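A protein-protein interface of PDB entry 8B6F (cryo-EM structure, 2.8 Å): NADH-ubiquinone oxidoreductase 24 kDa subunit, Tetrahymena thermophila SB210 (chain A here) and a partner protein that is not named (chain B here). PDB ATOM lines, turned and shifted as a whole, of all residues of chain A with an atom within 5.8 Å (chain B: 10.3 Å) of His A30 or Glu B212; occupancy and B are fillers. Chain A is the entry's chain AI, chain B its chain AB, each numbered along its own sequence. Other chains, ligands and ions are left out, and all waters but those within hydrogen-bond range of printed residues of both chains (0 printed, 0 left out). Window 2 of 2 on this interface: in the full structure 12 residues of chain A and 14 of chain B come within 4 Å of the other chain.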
ATOM      1  N   LEU A  27     -11.861   2.341  13.589  1.00  0.00           N
ATOM      2  CA  LEU A  27     -11.541   3.295  14.638  1.00  0.00           C
ATOM      3  C   LEU A  27     -11.753   4.718  14.142  1.00  0.00           C
ATOM      4  O   LEU A  27     -11.623   5.007  12.949  1.00  0.00           O
ATOM      5  CB  LEU A  27     -10.095   3.116  15.106  1.00  0.00           C
ATOM      6  CG  LEU A  27      -9.654   3.951  16.311  1.00  0.00           C
ATOM      7  CD1 LEU A  27     -10.448   3.579  17.554  1.00  0.00           C
ATOM      8  CD2 LEU A  27      -8.164   3.782  16.557  1.00  0.00           C
ATOM      9  N   ALA A  28     -12.082   5.613  15.075  1.00  0.00           N
ATOM     10  CA  ALA A  28     -12.275   7.026  14.775  1.00  0.00           C
ATOM     11  C   ALA A  28     -11.005   7.841  14.981  1.00  0.00           C
ATOM     12  O   ALA A  28     -11.080   9.040  15.281  1.00  0.00           O
ATOM     13  CB  ALA A  28     -13.413   7.591  15.626  1.00  0.00           C
ATOM     14  N   ALA A  29      -9.840   7.217  14.834  1.00  0.00           N
ATOM     15  CA  ALA A  29      -8.564   7.892  15.007  1.00  0.00           C
ATOM     16  C   ALA A  29      -7.519   7.150  14.186  1.00  0.00           C
ATOM     17  O   ALA A  29      -7.804   6.127  13.559  1.00  0.00           O
ATOM     18  CB  ALA A  29      -8.172   7.962  16.485  1.00  0.00           C
ATOM     19  N   HIS A  30      -6.297   7.674  14.194  1.00  0.00           N
ATOM     20  CA  HIS A  30      -5.221   7.076  13.415  1.00  0.00           C
ATOM     21  C   HIS A  30      -4.742   5.800  14.091  1.00  0.00           C
ATOM     22  O   HIS A  30      -4.301   5.828  15.245  1.00  0.00           O
ATOM     23  CB  HIS A  30      -4.067   8.062  13.258  1.00  0.00           C
ATOM     24  CG  HIS A  30      -2.933   7.530  12.440  1.00  0.00           C
ATOM     25  ND1 HIS A  30      -1.702   7.225  12.981  1.00  0.00           N
ATOM     26  CD2 HIS A  30      -2.846   7.237  11.122  1.00  0.00           C
ATOM     27  CE1 HIS A  30      -0.906   6.772  12.031  1.00  0.00           C
ATOM     28  NE2 HIS A  30      -1.575   6.769  10.892  1.00  0.00           N
ATOM     29  N   ARG A  31      -4.825   4.682  13.376  1.00  0.00           N
ATOM     30  CA  ARG A  31      -4.311   3.420  13.884  1.00  0.00           C
ATOM     31  C   ARG A  31      -2.797   3.391  13.730  1.00  0.00           C
ATOM     32  O   ARG A  31      -2.268   3.717  12.663  1.00  0.00           O
ATOM     33  CB  ARG A  31      -4.943   2.245  13.139  1.00  0.00           C
ATOM     34  CG  ARG A  31      -4.587   0.881  13.709  1.00  0.00           C
ATOM     35  CD  ARG A  31      -5.346   0.590  14.993  1.00  0.00           C
ATOM     36  NE  ARG A  31      -6.734   0.227  14.737  1.00  0.00           N
ATOM     37  CZ  ARG A  31      -7.567  -0.244  15.655  1.00  0.00           C
ATOM     38  NH1 ARG A  31      -7.183  -0.428  16.908  1.00  0.00           N
ATOM     39  NH2 ARG A  31      -8.815  -0.540  15.308  1.00  0.00           N
ATOM     40  N   LYS A  32      -2.103   2.997  14.795  1.00  0.00           N
ATOM     41  CA  LYS A  32      -0.646   2.973  14.787  1.00  0.00           C
ATOM     42  C   LYS A  32      -0.143   1.818  13.933  1.00  0.00           C
ATOM     43  O   LYS A  32      -0.030   0.685  14.413  1.00  0.00           O
ATOM     44  CB  LYS A  32      -0.109   2.860  16.215  1.00  0.00           C
ATOM     45  CG  LYS A  32       1.407   2.916  16.327  1.00  0.00           C
ATOM     46  CD  LYS A  32       1.952   4.261  15.878  1.00  0.00           C
ATOM     47  CE  LYS A  32       3.446   4.367  16.144  1.00  0.00           C
ATOM     48  NZ  LYS A  32       4.221   3.307  15.440  1.00  0.00           N
ATOM     49  N   ASN A  33       0.158   2.095  12.667  1.00  0.00           N
ATOM     50  CA  ASN A  33       0.634   1.095  11.725  1.00  0.00           C
ATOM     51  C   ASN A  33       1.976   1.530  11.157  1.00  0.00           C
ATOM     52  O   ASN A  33       2.196   2.718  10.902  1.00  0.00           O
ATOM     53  CB  ASN A  33      -0.372   0.882  10.592  1.00  0.00           C
ATOM     54  CG  ASN A  33       0.065  -0.192   9.619  1.00  0.00           C
ATOM     55  OD1 ASN A  33       0.982  -0.965   9.899  1.00  0.00           O
ATOM     56  ND2 ASN A  33      -0.593  -0.249   8.467  1.00  0.00           N
ATOM     57  N   ASN A  36       1.686   2.906   7.552  1.00  0.00           N
ATOM     58  CA  ASN A  36       0.890   4.115   7.383  1.00  0.00           C
ATOM     59  C   ASN A  36       1.466   5.258   8.208  1.00  0.00           C
ATOM     60  O   ASN A  36       0.743   6.174   8.606  1.00  0.00           O
ATOM     61  CB  ASN A  36      -0.569   3.861   7.760  1.00  0.00           C
ATOM     62  CG  ASN A  36      -1.484   4.987   7.330  1.00  0.00           C
ATOM     63  OD1 ASN A  36      -1.160   5.752   6.424  1.00  0.00           O
ATOM     64  ND2 ASN A  36      -2.637   5.094   7.980  1.00  0.00           N
ATOM     65  N   SER A  37       2.768   5.217   8.473  1.00  0.00           N
ATOM     66  CA  SER A  37       3.410   6.269   9.243  1.00  0.00           C
ATOM     67  C   SER A  37       3.504   7.547   8.413  1.00  0.00           C
ATOM     68  O   SER A  37       3.265   7.560   7.203  1.00  0.00           O
ATOM     69  CB  SER A  37       4.799   5.827   9.704  1.00  0.00           C
ATOM     70  OG  SER A  37       5.635   5.527   8.599  1.00  0.00           O
ATOM     71  N   LEU A  85      -2.266   8.475   5.433  1.00  0.00           N
ATOM     72  CA  LEU A  85      -2.224   9.714   6.204  1.00  0.00           C
ATOM     73  C   LEU A  85      -1.385  10.773   5.501  1.00  0.00           C
ATOM     74  O   LEU A  85      -1.729  11.960   5.516  1.00  0.00           O
ATOM     75  CB  LEU A  85      -1.680   9.440   7.606  1.00  0.00           C
ATOM     76  CG  LEU A  85      -1.625  10.643   8.551  1.00  0.00           C
ATOM     77  CD1 LEU A  85      -3.016  11.192   8.823  1.00  0.00           C
ATOM     78  CD2 LEU A  85      -0.941  10.260   9.851  1.00  0.00           C
ATOM     79  N   ARG A 114      -9.391   3.960   5.250  1.00  0.00           N
ATOM     80  CA  ARG A 114      -8.210   4.564   5.849  1.00  0.00           C
ATOM     81  C   ARG A 114      -7.076   3.570   6.054  1.00  0.00           C
ATOM     82  O   ARG A 114      -5.970   3.987   6.412  1.00  0.00           O
ATOM     83  CB  ARG A 114      -8.575   5.216   7.186  1.00  0.00           C
ATOM     84  CG  ARG A 114      -9.448   6.452   7.036  1.00  0.00           C
ATOM     85  CD  ARG A 114      -9.754   7.106   8.374  1.00  0.00           C
ATOM     86  NE  ARG A 114     -10.652   6.302   9.195  1.00  0.00           N
ATOM     87  CZ  ARG A 114     -10.261   5.411  10.098  1.00  0.00           C
ATOM     88  NH1 ARG A 114      -8.980   5.166  10.321  1.00  0.00           N
ATOM     89  NH2 ARG A 114     -11.180   4.748  10.794  1.00  0.00           N
ATOM     90  N   GLU B 162     -10.846   5.654  24.206  1.00  0.00           N
ATOM     91  CA  GLU B 162      -9.453   5.697  24.625  1.00  0.00           C
ATOM     92  C   GLU B 162      -9.046   7.121  24.985  1.00  0.00           C
ATOM     93  O   GLU B 162      -9.554   8.098  24.430  1.00  0.00           O
ATOM     94  CB  GLU B 162      -8.548   5.170  23.514  1.00  0.00           C
ATOM     95  CG  GLU B 162      -7.074   5.158  23.877  1.00  0.00           C
ATOM     96  CD  GLU B 162      -6.201   4.700  22.732  1.00  0.00           C
ATOM     97  OE1 GLU B 162      -6.751   4.209  21.725  1.00  0.00           O
ATOM     98  OE2 GLU B 162      -4.964   4.833  22.837  1.00  0.00           O
ATOM     99  N   ASP B 163      -8.116   7.230  25.930  1.00  0.00           N
ATOM    100  CA  ASP B 163      -7.610   8.526  26.345  1.00  0.00           C
ATOM    101  C   ASP B 163      -6.595   9.054  25.335  1.00  0.00           C
ATOM    102  O   ASP B 163      -6.070   8.319  24.495  1.00  0.00           O
ATOM    103  CB  ASP B 163      -6.968   8.439  27.730  1.00  0.00           C
ATOM    104  CG  ASP B 163      -7.971   8.105  28.816  1.00  0.00           C
ATOM    105  OD1 ASP B 163      -9.172   8.384  28.621  1.00  0.00           O
ATOM    106  OD2 ASP B 163      -7.559   7.569  29.866  1.00  0.00           O
ATOM    107  N   LYS B 164      -6.323  10.352  25.431  1.00  0.00           N
ATOM    108  CA  LYS B 164      -5.425  11.039  24.517  1.00  0.00           C
ATOM    109  C   LYS B 164      -4.421  11.863  25.310  1.00  0.00           C
ATOM    110  O   LYS B 164      -4.704  12.312  26.423  1.00  0.00           O
ATOM    111  CB  LYS B 164      -6.202  11.942  23.553  1.00  0.00           C
ATOM    112  CG  LYS B 164      -7.228  11.193  22.718  1.00  0.00           C
ATOM    113  CD  LYS B 164      -8.084  12.144  21.900  1.00  0.00           C
ATOM    114  CE  LYS B 164      -9.025  11.380  20.983  1.00  0.00           C
ATOM    115  NZ  LYS B 164      -9.922  10.455  21.731  1.00  0.00           N
ATOM    116  N   ASN B 165      -3.242  12.053  24.724  1.00  0.00           N
ATOM    117  CA  ASN B 165      -2.147  12.785  25.352  1.00  0.00           C
ATOM    118  C   ASN B 165      -2.045  14.154  24.690  1.00  0.00           C
ATOM    119  O   ASN B 165      -1.630  14.259  23.531  1.00  0.00           O
ATOM    120  CB  ASN B 165      -0.838  12.011  25.224  1.00  0.00           C
ATOM    121  CG  ASN B 165       0.290  12.635  26.017  1.00  0.00           C
ATOM    122  OD1 ASN B 165       0.298  13.840  26.266  1.00  0.00           O
ATOM    123  ND2 ASN B 165       1.253  11.815  26.421  1.00  0.00           N
ATOM    124  N   TYR B 166      -2.419  15.200  25.428  1.00  0.00           N
ATOM    125  CA  TYR B 166      -2.355  16.571  24.939  1.00  0.00           C
ATOM    126  C   TYR B 166      -1.229  17.375  25.580  1.00  0.00           C
ATOM    127  O   TYR B 166      -1.181  18.596  25.407  1.00  0.00           O
ATOM    128  CB  TYR B 166      -3.689  17.284  25.174  1.00  0.00           C
ATOM    129  CG  TYR B 166      -4.840  16.787  24.321  1.00  0.00           C
ATOM    130  CD1 TYR B 166      -4.652  15.813  23.348  1.00  0.00           C
ATOM    131  CD2 TYR B 166      -6.115  17.312  24.482  1.00  0.00           C
ATOM    132  CE1 TYR B 166      -5.701  15.370  22.570  1.00  0.00           C
ATOM    133  CE2 TYR B 166      -7.170  16.875  23.709  1.00  0.00           C
ATOM    134  CZ  TYR B 166      -6.957  15.905  22.755  1.00  0.00           C
ATOM    135  OH  TYR B 166      -8.007  15.469  21.982  1.00  0.00           O
ATOM    136  N   GLY B 167      -0.329  16.727  26.314  1.00  0.00           N
ATOM    137  CA  GLY B 167       0.777  17.413  26.938  1.00  0.00           C
ATOM    138  C   GLY B 167       0.649  17.464  28.445  1.00  0.00           C
ATOM    139  O   GLY B 167      -0.302  16.936  29.030  1.00  0.00           O
ATOM    140  N   ASP B 195      -6.369  22.091  15.668  1.00  0.00           N
ATOM    141  CA  ASP B 195      -5.976  20.711  15.933  1.00  0.00           C
ATOM    142  C   ASP B 195      -7.142  19.829  16.347  1.00  0.00           C
ATOM    143  O   ASP B 195      -7.166  18.649  15.989  1.00  0.00           O
ATOM    144  CB  ASP B 195      -4.899  20.680  17.028  1.00  0.00           C
ATOM    145  CG  ASP B 195      -3.684  21.511  16.673  1.00  0.00           C
ATOM    146  OD1 ASP B 195      -3.399  21.663  15.466  1.00  0.00           O
ATOM    147  OD2 ASP B 195      -3.014  22.013  17.601  1.00  0.00           O
ATOM    148  N   LEU B 196      -8.105  20.366  17.087  1.00  0.00           N
ATOM    149  CA  LEU B 196      -9.206  19.574  17.611  1.00  0.00           C
ATOM    150  C   LEU B 196     -10.354  19.530  16.613  1.00  0.00           C
ATOM    151  O   LEU B 196     -10.661  20.525  15.953  1.00  0.00           O
ATOM    152  CB  LEU B 196      -9.690  20.150  18.943  1.00  0.00           C
ATOM    153  CG  LEU B 196      -8.596  20.379  19.990  1.00  0.00           C
ATOM    154  CD1 LEU B 196      -9.189  20.938  21.269  1.00  0.00           C
ATOM    155  CD2 LEU B 196      -7.831  19.098  20.270  1.00  0.00           C
ATOM    156  N   THR B 199     -13.932  13.796  14.909  1.00  0.00           N
ATOM    157  CA  THR B 199     -13.636  12.750  13.940  1.00  0.00           C
ATOM    158  C   THR B 199     -14.509  11.532  14.211  1.00  0.00           C
ATOM    159  O   THR B 199     -14.525  11.008  15.328  1.00  0.00           O
ATOM    160  CB  THR B 199     -12.157  12.364  13.997  1.00  0.00           C
ATOM    161  OG1 THR B 199     -11.790  12.051  15.348  1.00  0.00           O
ATOM    162  CG2 THR B 199     -11.289  13.501  13.484  1.00  0.00           C
ATOM    163  N   GLY B 200     -15.227  11.089  13.190  1.00  0.00           N
ATOM    164  CA  GLY B 200     -16.103   9.940  13.287  1.00  0.00           C
ATOM    165  C   GLY B 200     -17.563  10.322  13.113  1.00  0.00           C
ATOM    166  O   GLY B 200     -17.934  11.492  13.017  1.00  0.00           O
ATOM    167  N   GLU B 206     -15.466  10.930  18.048  1.00  0.00           N
ATOM    168  CA  GLU B 206     -14.480  11.289  19.059  1.00  0.00           C
ATOM    169  C   GLU B 206     -13.936  12.674  18.752  1.00  0.00           C
ATOM    170  O   GLU B 206     -13.355  12.894  17.685  1.00  0.00           O
ATOM    171  CB  GLU B 206     -13.340  10.267  19.101  1.00  0.00           C
ATOM    172  CG  GLU B 206     -13.797   8.854  19.411  1.00  0.00           C
ATOM    173  CD  GLU B 206     -12.660   7.857  19.374  1.00  0.00           C
ATOM    174  OE1 GLU B 206     -11.527   8.260  19.038  1.00  0.00           O
ATOM    175  OE2 GLU B 206     -12.897   6.670  19.683  1.00  0.00           O
ATOM    176  N   GLY B 208     -11.239  15.419  19.126  1.00  0.00           N
ATOM    177  CA  GLY B 208      -9.828  15.488  19.433  1.00  0.00           C
ATOM    178  C   GLY B 208      -9.006  15.412  18.163  1.00  0.00           C
ATOM    179  O   GLY B 208      -9.534  15.426  17.057  1.00  0.00           O
ATOM    180  N   THR B 209      -7.693  15.333  18.355  1.00  0.00           N
ATOM    181  CA  THR B 209      -6.766  15.230  17.239  1.00  0.00           C
ATOM    182  C   THR B 209      -6.804  13.820  16.666  1.00  0.00           C
ATOM    183  O   THR B 209      -6.719  12.837  17.406  1.00  0.00           O
ATOM    184  CB  THR B 209      -5.347  15.579  17.683  1.00  0.00           C
ATOM    185  OG1 THR B 209      -4.909  14.647  18.679  1.00  0.00           O
ATOM    186  CG2 THR B 209      -5.294  16.988  18.255  1.00  0.00           C
ATOM    187  N   TYR B 210      -6.938  13.724  15.342  1.00  0.00           N
ATOM    188  CA  TYR B 210      -6.920  12.418  14.694  1.00  0.00           C
ATOM    189  C   TYR B 210      -5.579  11.726  14.899  1.00  0.00           C
ATOM    190  O   TYR B 210      -5.528  10.533  15.220  1.00  0.00           O
ATOM    191  CB  TYR B 210      -7.226  12.580  13.206  1.00  0.00           C
ATOM    192  CG  TYR B 210      -7.146  11.304  12.403  1.00  0.00           C
ATOM    193  CD1 TYR B 210      -8.180  10.377  12.426  1.00  0.00           C
ATOM    194  CD2 TYR B 210      -6.045  11.039  11.601  1.00  0.00           C
ATOM    195  CE1 TYR B 210      -8.112   9.215  11.683  1.00  0.00           C
ATOM    196  CE2 TYR B 210      -5.967   9.881  10.856  1.00  0.00           C
ATOM    197  CZ  TYR B 210      -7.003   8.974  10.900  1.00  0.00           C
ATOM    198  OH  TYR B 210      -6.923   7.821  10.156  1.00  0.00           O
ATOM    199  N   VAL B 211      -4.485  12.461  14.726  1.00  0.00           N
ATOM    200  CA  VAL B 211      -3.153  11.933  14.972  1.00  0.00           C
ATOM    201  C   VAL B 211      -2.777  12.197  16.424  1.00  0.00           C
ATOM    202  O   VAL B 211      -3.384  13.023  17.111  1.00  0.00           O
ATOM    203  CB  VAL B 211      -2.114  12.539  14.008  1.00  0.00           C
ATOM    204  CG1 VAL B 211      -2.495  12.248  12.566  1.00  0.00           C
ATOM    205  CG2 VAL B 211      -1.978  14.040  14.232  1.00  0.00           C
ATOM    206  N   GLU B 212      -1.759  11.487  16.900  1.00  0.00           N
ATOM    207  CA  GLU B 212      -1.297  11.620  18.280  1.00  0.00           C
ATOM    208  C   GLU B 212      -0.318  12.787  18.353  1.00  0.00           C
ATOM    209  O   GLU B 212       0.852  12.657  17.986  1.00  0.00           O
ATOM    210  CB  GLU B 212      -0.660  10.323  18.772  1.00  0.00           C
ATOM    211  CG  GLU B 212       0.363   9.701  17.825  1.00  0.00           C
ATOM    212  CD  GLU B 212      -0.263   8.743  16.825  1.00  0.00           C
ATOM    213  OE1 GLU B 212      -1.507   8.679  16.753  1.00  0.00           O
ATOM    214  OE2 GLU B 212       0.494   8.051  16.113  1.00  0.00           O
ATOM    215  N   LYS B 213      -0.799  13.931  18.834  1.00  0.00           N
ATOM    216  CA  LYS B 213       0.041  15.107  19.002  1.00  0.00           C
ATOM    217  C   LYS B 213      -0.466  15.905  20.193  1.00  0.00           C
ATOM    218  O   LYS B 213      -1.616  15.769  20.614  1.00  0.00           O
ATOM    219  CB  LYS B 213       0.060  15.974  17.737  1.00  0.00           C
ATOM    220  CG  LYS B 213      -1.296  16.533  17.339  1.00  0.00           C
ATOM    221  CD  LYS B 213      -1.199  17.315  16.038  1.00  0.00           C
ATOM    222  CE  LYS B 213      -2.564  17.791  15.573  1.00  0.00           C
ATOM    223  NZ  LYS B 213      -2.494  18.469  14.247  1.00  0.00           N
ATOM    224  N   THR B 214       0.415  16.743  20.733  1.00  0.00           N
ATOM    225  CA  THR B 214       0.120  17.510  21.934  1.00  0.00           C
ATOM    226  C   THR B 214      -0.487  18.860  21.580  1.00  0.00           C
ATOM    227  O   THR B 214      -0.124  19.476  20.574  1.00  0.00           O
ATOM    228  CB  THR B 214       1.387  17.716  22.766  1.00  0.00           C
ATOM    229  OG1 THR B 214       2.387  18.364  21.972  1.00  0.00           O
ATOM    230  CG2 THR B 214       1.921  16.382  23.266  1.00  0.00           C
ATOM    231  N   PHE B 215      -1.414  19.316  22.420  1.00  0.00           N
ATOM    232  CA  PHE B 215      -2.061  20.618  22.259  1.00  0.00           C
ATOM    233  C   PHE B 215      -1.212  21.640  23.007  1.00  0.00           C
ATOM    234  O   PHE B 215      -1.393  21.879  24.201  1.00  0.00           O
ATOM    235  CB  PHE B 215      -3.492  20.565  22.779  1.00  0.00           C
ATOM    236  CG  PHE B 215      -4.328  21.742  22.375  1.00  0.00           C
ATOM    237  CD1 PHE B 215      -4.756  21.886  21.066  1.00  0.00           C
ATOM    238  CD2 PHE B 215      -4.705  22.691  23.307  1.00  0.00           C
ATOM    239  CE1 PHE B 215      -5.531  22.965  20.690  1.00  0.00           C
ATOM    240  CE2 PHE B 215      -5.480  23.772  22.938  1.00  0.00           C
ATOM    241  CZ  PHE B 215      -5.894  23.908  21.629  1.00  0.00           C
ATOM    242  N   ASN B 216      -0.270  22.255  22.290  1.00  0.00           N
ATOM    243  CA  ASN B 216       0.779  23.068  22.897  1.00  0.00           C
ATOM    244  C   ASN B 216       0.552  24.565  22.713  1.00  0.00           C
ATOM    245  O   ASN B 216       1.506  25.344  22.801  1.00  0.00           O
ATOM    246  CB  ASN B 216       2.143  22.675  22.330  1.00  0.00           C
ATOM    247  CG  ASN B 216       2.219  22.836  20.824  1.00  0.00           C
ATOM    248  OD1 ASN B 216       1.359  23.465  20.211  1.00  0.00           O
ATOM    249  ND2 ASN B 216       3.256  22.268  20.223  1.00  0.00           N
ATOM    250  N   GLU B 708       9.179  20.824  20.017  1.00  0.00           N
ATOM    251  CA  GLU B 708       8.072  20.773  19.070  1.00  0.00           C
ATOM    252  C   GLU B 708       7.740  22.145  18.499  1.00  0.00           C
ATOM    253  O   GLU B 708       7.245  22.236  17.370  1.00  0.00           O
ATOM    254  CB  GLU B 708       6.836  20.176  19.747  1.00  0.00           C
ATOM    255  CG  GLU B 708       5.669  19.913  18.809  1.00  0.00           C
ATOM    256  CD  GLU B 708       5.967  18.824  17.793  1.00  0.00           C
ATOM    257  OE1 GLU B 708       7.055  18.215  17.871  1.00  0.00           O
ATOM    258  OE2 GLU B 708       5.110  18.574  16.919  1.00  0.00           O
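The backbone NH (N) of Leu A85 sits at hydrogen-bond distance from the side-chain amide oxygen (OD1) of Asn A36. OE1 of Glu B206 is in salt-bridge range of NZ of Lys B164 (3.8 Å). The backbone carbonyl oxygen (O) of Asn A36 sits at hydrogen-bond distance from a ring nitrogen (NE2) of His A30, 3.3 Å away. O of Thr B199 is in hydrogen-bond range of N of Glu B206. The side-chain hydroxyl (OG1) of Thr B209 sits at hydrogen-bond distance from the backbone carbonyl oxygen (O) of Val B211, 2.7 Å away.
Among the printed residues, pairs that only touch across the chains: Ala A28 with Glu B206 (3.8 Å), Ala A29 with Tyr B210 (3.3 Å), His A30 with Glu B212 (3.9 Å), Leu A85 with Tyr B210 (3.8 Å) and Leu A85 with Val B211 (3.7 Å).
Of chain B, only Tyr B210 (3.1 Å) and Glu B212 (3.9 Å) come within 4 Å of His A30. Glu B212 touches one residue of chain A. Of the printed residues of chain A, Tyr B210 touches Ala A29, His A30, Leu A85 and Arg A114. Of the printed residues of chain B, Leu A85 touches Tyr B210 and Val B211. Of the printed residues of chain A, Val B211 touches Leu A85. Printed residues of chain A within 4 Å of Thr B199: Ala A28. Printed residues of chain B within 4 Å of Arg A114: Tyr B210 (3.4 Å). Glu B708 touches none of the printed residues of chain A. The nearest printed residue of chain B that does not touch Arg A114 is Gly B200 (7.6 Å).
The guanidinium group (NH1) of Arg A114 sits at hydrogen-bond distance from the side-chain hydroxyl (OH) of Tyr B210 (3.4 Å). OG1 of Thr B199 is in hydrogen-bond range of O of Ala A28 (3.1 Å). The backbone NH (N) of His A30 is in hydrogen-bond range of the backbone carbonyl oxygen (O) of Tyr B210 (3.1 Å).
Of the 21 printed residues of chain B, 5 touch a printed residue of chain A. Along chain B the printed residues that touch a printed residue of chain A span positions 199 to 212. Hydrophobic or aromatic side chains of chain A that line the printed part of chain B: Ala A28, Ala A29, His A30 and Leu A85.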
